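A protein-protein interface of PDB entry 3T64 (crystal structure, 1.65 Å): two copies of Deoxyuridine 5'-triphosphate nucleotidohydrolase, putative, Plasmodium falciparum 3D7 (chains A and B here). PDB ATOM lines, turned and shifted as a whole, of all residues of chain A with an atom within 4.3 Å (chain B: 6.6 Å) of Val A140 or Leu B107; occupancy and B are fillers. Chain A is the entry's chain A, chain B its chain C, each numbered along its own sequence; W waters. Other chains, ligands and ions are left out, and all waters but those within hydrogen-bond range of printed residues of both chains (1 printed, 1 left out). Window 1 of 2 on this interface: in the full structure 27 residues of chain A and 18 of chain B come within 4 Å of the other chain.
OG of Ser A27 is in hydrogen-bond range of OG of Ser B85 (3.4 Å).
The side-chain carboxylate (OD1) of Asp B109 sits at hydrogen-bond distance from the backbone NH (N) of Ser A27.
The backbone carbonyl oxygen (O) of Phe A89 sits at hydrogen-bond distance from the backbone NH (N) of Gln A138, 2.8 Å away.
The side-chain sulfur (SD) of Met A1 sits close to the side-chain hydroxyl (OG) of Ser A141, at 3.7 Å.
The backbone carbonyl oxygen (O) of Leu A87 sits at hydrogen-bond distance from the backbone NH (N) of Val A140 (2.9 Å).
Among the printed residues, merely in contact across the chains: Phe A89 with Leu B87 (3.8 Å), Phe A89 with Ile B105 (3.8 Å), Gln A138 with Leu B107 (3.8 Å), Val A140 with Leu B107 (3.9 Å), Val A140 with Phe B142 (3.9 Å), Ser A141 with Phe B142 (3.6 Å) and Phe A142 with Phe B142 (3.3 Å).
Phe A86 touches none of the printed residues of chain B.
Of the printed residues of chain B, Phe A89 touches Leu B87 (3.8 Å) and Ile B105 (3.8 Å).
Val A140 touches two residues of chain B.
Of the printed residues of chain A, Ser B85 touches Ser A27 (3.4 Å).
Leu B88 touches none of the printed residues of chain A.
Of the printed residues of chain A, Leu B107 touches Gln A138 and Val A140.
The nearest residue of chain B that does not touch Val A140 is Leu B87 (6.2 Å).
Printed residues of chain A that touch a printed residue of chain B: Ser A27, Phe A89, Gln A138, Val A140, Ser A141 and Phe A142.
Hydrophobic or aromatic side chains of chain A within 4 Å of the printed part of chain B: Phe A89 and Val A140.
Of the 11 printed residues of chain B, 6 touch a printed residue of chain A.
Hydrophobic or aromatic side chains of chain B within 4 Å of the printed part of chain A: Leu B87, Ile B105, Leu B107 and Phe B142.
Among the printed residues, 9 pairs touch across the chains.
Phe A142 touches its own counterpart, Phe B142.
Positions printed for both chains: 86, 87 and 142.
Of the 9 pairs that touch across the chains among the printed residues, 1 has its exchanged pair printed and touching as well.
Water W1 lies within hydrogen-bond range of OD2 of Asp B109 (2.6 Å), N of Gly A28 (3.1 Å) and N of Ser A27 (3.5 Å).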
ATOM      1  N   MET A   1      35.238  29.743 -28.537  1.00  0.00           N
ATOM      2  CA  MET A   1      35.190  28.360 -29.113  1.00  0.00           C
ATOM      3  C   MET A   1      34.579  28.420 -30.498  1.00  0.00           C
ATOM      4  O   MET A   1      33.594  29.124 -30.708  1.00  0.00           O
ATOM      5  CB  MET A   1      34.351  27.433 -28.224  1.00  0.00           C
ATOM      6  CG  MET A   1      34.426  25.965 -28.638  1.00  0.00           C
ATOM      7  SD  MET A   1      33.579  24.854 -27.499  1.00  0.00           S
ATOM      8  CE  MET A   1      31.906  25.012 -28.074  1.00  0.00           C
ATOM      9  N   SER A  27      27.016  32.466 -25.682  1.00  0.00           N
ATOM     10  CA  SER A  27      27.673  31.291 -25.097  1.00  0.00           C
ATOM     11  C   SER A  27      27.028  29.983 -25.511  1.00  0.00           C
ATOM     12  O   SER A  27      27.614  28.922 -25.344  1.00  0.00           O
ATOM     13  CB  SER A  27      27.678  31.386 -23.567  1.00  0.00           C
ATOM     14  OG  SER A  27      28.650  32.329 -23.177  1.00  0.00           O
ATOM     15  N   GLY A  28      25.832  30.053 -26.077  1.00  0.00           N
ATOM     16  CA  GLY A  28      25.196  28.826 -26.571  1.00  0.00           C
ATOM     17  C   GLY A  28      24.780  28.941 -28.005  1.00  0.00           C
ATOM     18  O   GLY A  28      24.373  30.026 -28.458  1.00  0.00           O
ATOM     19  N   PHE A  86      32.999  19.292 -25.739  1.00  0.00           N
ATOM     20  CA  PHE A  86      32.041  20.386 -25.568  1.00  0.00           C
ATOM     21  C   PHE A  86      30.757  19.830 -24.998  1.00  0.00           C
ATOM     22  O   PHE A  86      30.659  18.621 -24.787  1.00  0.00           O
ATOM     23  CB  PHE A  86      31.792  21.167 -26.873  1.00  0.00           C
ATOM     24  CG  PHE A  86      31.360  20.323 -28.039  1.00  0.00           C
ATOM     25  CD1 PHE A  86      32.287  19.587 -28.773  1.00  0.00           C
ATOM     26  CD2 PHE A  86      30.028  20.297 -28.441  1.00  0.00           C
ATOM     27  CE1 PHE A  86      31.903  18.821 -29.851  1.00  0.00           C
ATOM     28  CE2 PHE A  86      29.627  19.546 -29.541  1.00  0.00           C
ATOM     29  CZ  PHE A  86      30.557  18.789 -30.247  1.00  0.00           C
ATOM     30  N   LEU A  87      29.789  20.710 -24.750  1.00  0.00           N
ATOM     31  CA  LEU A  87      28.600  20.306 -23.975  1.00  0.00           C
ATOM     32  C   LEU A  87      27.309  20.496 -24.746  1.00  0.00           C
ATOM     33  O   LEU A  87      27.173  21.407 -25.579  1.00  0.00           O
ATOM     34  CB  LEU A  87      28.549  21.094 -22.666  1.00  0.00           C
ATOM     35  CG  LEU A  87      29.798  20.893 -21.789  1.00  0.00           C
ATOM     36  CD1 LEU A  87      29.924  21.961 -20.742  1.00  0.00           C
ATOM     37  CD2 LEU A  87      29.715  19.491 -21.116  1.00  0.00           C
ATOM     38  N   PHE A  89      23.546  21.339 -23.808  1.00  0.00           N
ATOM     39  CA  PHE A  89      22.639  21.815 -22.748  1.00  0.00           C
ATOM     40  C   PHE A  89      21.213  21.808 -23.279  1.00  0.00           C
ATOM     41  O   PHE A  89      20.979  22.135 -24.448  1.00  0.00           O
ATOM     42  CB  PHE A  89      22.910  23.289 -22.404  1.00  0.00           C
ATOM     43  CG  PHE A  89      23.932  23.514 -21.332  1.00  0.00           C
ATOM     44  CD1 PHE A  89      25.236  23.059 -21.486  1.00  0.00           C
ATOM     45  CD2 PHE A  89      23.613  24.297 -20.220  1.00  0.00           C
ATOM     46  CE1 PHE A  89      26.203  23.309 -20.503  1.00  0.00           C
ATOM     47  CE2 PHE A  89      24.568  24.548 -19.230  1.00  0.00           C
ATOM     48  CZ  PHE A  89      25.860  24.066 -19.370  1.00  0.00           C
ATOM     49  N   GLN A 138      21.155  23.189 -27.035  1.00  0.00           N
ATOM     50  CA  GLN A 138      22.168  24.109 -27.556  1.00  0.00           C
ATOM     51  C   GLN A 138      23.538  23.541 -27.243  1.00  0.00           C
ATOM     52  O   GLN A 138      23.698  22.806 -26.259  1.00  0.00           O
ATOM     53  CB  GLN A 138      21.991  25.496 -26.891  1.00  0.00           C
ATOM     54  CG  GLN A 138      22.073  25.459 -25.352  1.00  0.00           C
ATOM     55  CD  GLN A 138      21.722  26.800 -24.704  1.00  0.00           C
ATOM     56  OE1 GLN A 138      22.083  27.857 -25.220  1.00  0.00           O
ATOM     57  NE2 GLN A 138      21.055  26.760 -23.539  1.00  0.00           N
ATOM     58  N   LEU A 139      24.535  23.884 -28.070  1.00  0.00           N
ATOM     59  CA  LEU A 139      25.908  23.543 -27.757  1.00  0.00           C
ATOM     60  C   LEU A 139      26.579  24.640 -26.949  1.00  0.00           C
ATOM     61  O   LEU A 139      26.314  25.819 -27.176  1.00  0.00           O
ATOM     62  CB  LEU A 139      26.705  23.255 -29.043  1.00  0.00           C
ATOM     63  CG  LEU A 139      26.151  22.083 -29.846  1.00  0.00           C
ATOM     64  CD1 LEU A 139      26.950  21.899 -31.155  1.00  0.00           C
ATOM     65  CD2 LEU A 139      26.203  20.773 -29.018  1.00  0.00           C
ATOM     66  N   VAL A 140      27.471  24.250 -26.042  1.00  0.00           N
ATOM     67  CA  VAL A 140      28.109  25.198 -25.114  1.00  0.00           C
ATOM     68  C   VAL A 140      29.552  24.784 -24.915  1.00  0.00           C
ATOM     69  O   VAL A 140      29.862  23.600 -24.932  1.00  0.00           O
ATOM     70  CB  VAL A 140      27.350  25.214 -23.736  1.00  0.00           C
ATOM     71  CG1 VAL A 140      27.982  26.186 -22.747  1.00  0.00           C
ATOM     72  CG2 VAL A 140      25.838  25.579 -23.924  1.00  0.00           C
ATOM     73  N   SER A 141      30.440  25.769 -24.756  1.00  0.00           N
ATOM     74  CA  SER A 141      31.823  25.494 -24.420  1.00  0.00           C
ATOM     75  C   SER A 141      31.979  25.192 -22.937  1.00  0.00           C
ATOM     76  O   SER A 141      31.295  25.773 -22.105  1.00  0.00           O
ATOM     77  CB  SER A 141      32.697  26.720 -24.768  1.00  0.00           C
ATOM     78  OG  SER A 141      34.002  26.547 -24.218  1.00  0.00           O
ATOM     79  N   PHE A 142      32.931  24.323 -22.598  1.00  0.00           N
ATOM     80  CA  PHE A 142      33.295  24.134 -21.197  1.00  0.00           C
ATOM     81  C   PHE A 142      33.656  25.439 -20.476  1.00  0.00           C
ATOM     82  O   PHE A 142      33.401  25.586 -19.292  1.00  0.00           O
ATOM     83  CB  PHE A 142      34.425  23.105 -21.051  1.00  0.00           C
ATOM     84  CG  PHE A 142      33.948  21.708 -20.808  1.00  0.00           C
ATOM     85  CD1 PHE A 142      33.660  21.286 -19.513  1.00  0.00           C
ATOM     86  CD2 PHE A 142      33.820  20.801 -21.863  1.00  0.00           C
ATOM     87  CE1 PHE A 142      33.225  19.982 -19.273  1.00  0.00           C
ATOM     88  CE2 PHE A 142      33.396  19.497 -21.632  1.00  0.00           C
ATOM     89  CZ  PHE A 142      33.096  19.084 -20.334  1.00  0.00           C
ATOM     90  N   SER B  85      29.440  34.891 -18.845  1.00  0.00           N
ATOM     91  CA  SER B  85      28.365  33.927 -18.645  1.00  0.00           C
ATOM     92  C   SER B  85      28.553  33.179 -17.327  1.00  0.00           C
ATOM     93  O   SER B  85      29.674  33.059 -16.829  1.00  0.00           O
ATOM     94  CB  SER B  85      28.373  32.909 -19.781  1.00  0.00           C
ATOM     95  OG  SER B  85      29.643  32.297 -19.904  1.00  0.00           O
ATOM     96  N   PHE B  86      27.456  32.660 -16.769  1.00  0.00           N
ATOM     97  CA  PHE B  86      27.589  31.862 -15.541  1.00  0.00           C
ATOM     98  C   PHE B  86      26.439  30.872 -15.474  1.00  0.00           C
ATOM     99  O   PHE B  86      25.609  30.842 -16.385  1.00  0.00           O
ATOM    100  CB  PHE B  86      27.718  32.740 -14.269  1.00  0.00           C
ATOM    101  CG  PHE B  86      26.582  33.695 -14.042  1.00  0.00           C
ATOM    102  CD1 PHE B  86      26.482  34.888 -14.756  1.00  0.00           C
ATOM    103  CD2 PHE B  86      25.588  33.405 -13.106  1.00  0.00           C
ATOM    104  CE1 PHE B  86      25.425  35.766 -14.538  1.00  0.00           C
ATOM    105  CE2 PHE B  86      24.516  34.302 -12.875  1.00  0.00           C
ATOM    106  CZ  PHE B  86      24.446  35.484 -13.593  1.00  0.00           C
ATOM    107  N   LEU B  87      26.412  30.060 -14.415  1.00  0.00           N
ATOM    108  CA  LEU B  87      25.508  28.899 -14.365  1.00  0.00           C
ATOM    109  C   LEU B  87      24.628  28.890 -13.132  1.00  0.00           C
ATOM    110  O   LEU B  87      25.014  29.376 -12.057  1.00  0.00           O
ATOM    111  CB  LEU B  87      26.323  27.602 -14.392  1.00  0.00           C
ATOM    112  CG  LEU B  87      27.210  27.406 -15.640  1.00  0.00           C
ATOM    113  CD1 LEU B  87      28.405  26.471 -15.374  1.00  0.00           C
ATOM    114  CD2 LEU B  87      26.380  26.908 -16.810  1.00  0.00           C
ATOM    115  N   LEU B  88      23.428  28.342 -13.314  1.00  0.00           N
ATOM    116  CA  LEU B  88      22.483  28.092 -12.233  1.00  0.00           C
ATOM    117  C   LEU B  88      22.371  26.569 -12.034  1.00  0.00           C
ATOM    118  O   LEU B  88      21.865  25.856 -12.894  1.00  0.00           O
ATOM    119  CB  LEU B  88      21.115  28.708 -12.569  1.00  0.00           C
ATOM    120  CG  LEU B  88      20.054  28.568 -11.479  1.00  0.00           C
ATOM    121  CD1 LEU B  88      20.422  29.390 -10.256  1.00  0.00           C
ATOM    122  CD2 LEU B  88      18.669  28.984 -12.030  1.00  0.00           C
ATOM    123  N   ASN B 103      15.401  22.557 -16.694  1.00  0.00           N
ATOM    124  CA  ASN B 103      16.378  22.697 -17.780  1.00  0.00           C
ATOM    125  C   ASN B 103      17.766  22.179 -17.422  1.00  0.00           C
ATOM    126  O   ASN B 103      18.743  22.535 -18.083  1.00  0.00           O
ATOM    127  CB  ASN B 103      16.461  24.172 -18.264  1.00  0.00           C
ATOM    128  CG  ASN B 103      16.715  25.164 -17.139  1.00  0.00           C
ATOM    129  OD1 ASN B 103      16.256  24.996 -16.001  1.00  0.00           O
ATOM    130  ND2 ASN B 103      17.433  26.248 -17.471  1.00  0.00           N
ATOM    131  N   ILE B 105      20.624  22.484 -15.973  1.00  0.00           N
ATOM    132  CA  ILE B 105      21.538  23.526 -15.488  1.00  0.00           C
ATOM    133  C   ILE B 105      21.183  24.772 -16.293  1.00  0.00           C
ATOM    134  O   ILE B 105      21.052  24.691 -17.507  1.00  0.00           O
ATOM    135  CB  ILE B 105      23.028  23.157 -15.781  1.00  0.00           C
ATOM    136  CG1 ILE B 105      23.405  21.800 -15.139  1.00  0.00           C
ATOM    137  CG2 ILE B 105      23.985  24.270 -15.329  1.00  0.00           C
ATOM    138  CD1 ILE B 105      23.519  21.812 -13.599  1.00  0.00           C
ATOM    139  N   GLY B 106      21.049  25.900 -15.612  1.00  0.00           N
ATOM    140  CA  GLY B 106      20.685  27.152 -16.277  1.00  0.00           C
ATOM    141  C   GLY B 106      21.925  27.850 -16.789  1.00  0.00           C
ATOM    142  O   GLY B 106      22.966  27.881 -16.116  1.00  0.00           O
ATOM    143  N   LEU B 107      21.812  28.407 -17.986  1.00  0.00           N
ATOM    144  CA  LEU B 107      22.904  29.153 -18.616  1.00  0.00           C
ATOM    145  C   LEU B 107      22.510  30.625 -18.654  1.00  0.00           C
ATOM    146  O   LEU B 107      21.528  31.004 -19.278  1.00  0.00           O
ATOM    147  CB  LEU B 107      23.184  28.624 -20.032  1.00  0.00           C
ATOM    148  CG  LEU B 107      24.197  29.380 -20.900  1.00  0.00           C
ATOM    149  CD1 LEU B 107      25.537  29.462 -20.236  1.00  0.00           C
ATOM    150  CD2 LEU B 107      24.334  28.749 -22.283  1.00  0.00           C
ATOM    151  N   ILE B 108      23.277  31.453 -17.955  1.00  0.00           N
ATOM    152  CA  ILE B 108      23.001  32.896 -17.946  1.00  0.00           C
ATOM    153  C   ILE B 108      24.096  33.578 -18.763  1.00  0.00           C
ATOM    154  O   ILE B 108      25.253  33.549 -18.374  1.00  0.00           O
ATOM    155  CB  ILE B 108      22.921  33.439 -16.508  1.00  0.00           C
ATOM    156  CG1 ILE B 108      21.881  32.638 -15.719  1.00  0.00           C
ATOM    157  CG2 ILE B 108      22.543  34.940 -16.535  1.00  0.00           C
ATOM    158  CD1 ILE B 108      21.893  32.870 -14.275  1.00  0.00           C
ATOM    159  N   ASP B 109      23.749  34.147 -19.923  1.00  0.00           N
ATOM    160  CA  ASP B 109      24.794  34.674 -20.808  1.00  0.00           C
ATOM    161  C   ASP B 109      25.357  35.977 -20.261  1.00  0.00           C
ATOM    162  O   ASP B 109      24.667  36.671 -19.514  1.00  0.00           O
ATOM    163  CB  ASP B 109      24.259  34.917 -22.223  1.00  0.00           C
ATOM    164  CG  ASP B 109      24.584  33.778 -23.175  1.00  0.00           C
ATOM    165  OD1 ASP B 109      25.532  33.950 -23.965  1.00  0.00           O
ATOM    166  OD2 ASP B 109      23.907  32.716 -23.123  1.00  0.00           O
ATOM    167  N   PHE B 142      31.681  29.054 -14.672  1.00  0.00           N
ATOM    168  CA  PHE B 142      32.161  28.052 -15.630  1.00  0.00           C
ATOM    169  C   PHE B 142      33.520  27.419 -15.292  1.00  0.00           C
ATOM    170  O   PHE B 142      33.798  26.291 -15.689  1.00  0.00           O
ATOM    171  CB  PHE B 142      32.208  28.658 -17.040  1.00  0.00           C
ATOM    172  CG  PHE B 142      30.926  28.510 -17.820  1.00  0.00           C
ATOM    173  CD1 PHE B 142      30.672  27.342 -18.552  1.00  0.00           C
ATOM    174  CD2 PHE B 142      29.982  29.534 -17.843  1.00  0.00           C
ATOM    175  CE1 PHE B 142      29.503  27.211 -19.308  1.00  0.00           C
ATOM    176  CE2 PHE B 142      28.798  29.414 -18.588  1.00  0.00           C
ATOM    177  CZ  PHE B 142      28.559  28.232 -19.330  1.00  0.00           C
HETATM  178  O   HOH W   1      23.556  32.022 -25.579  1.00  0.00           O
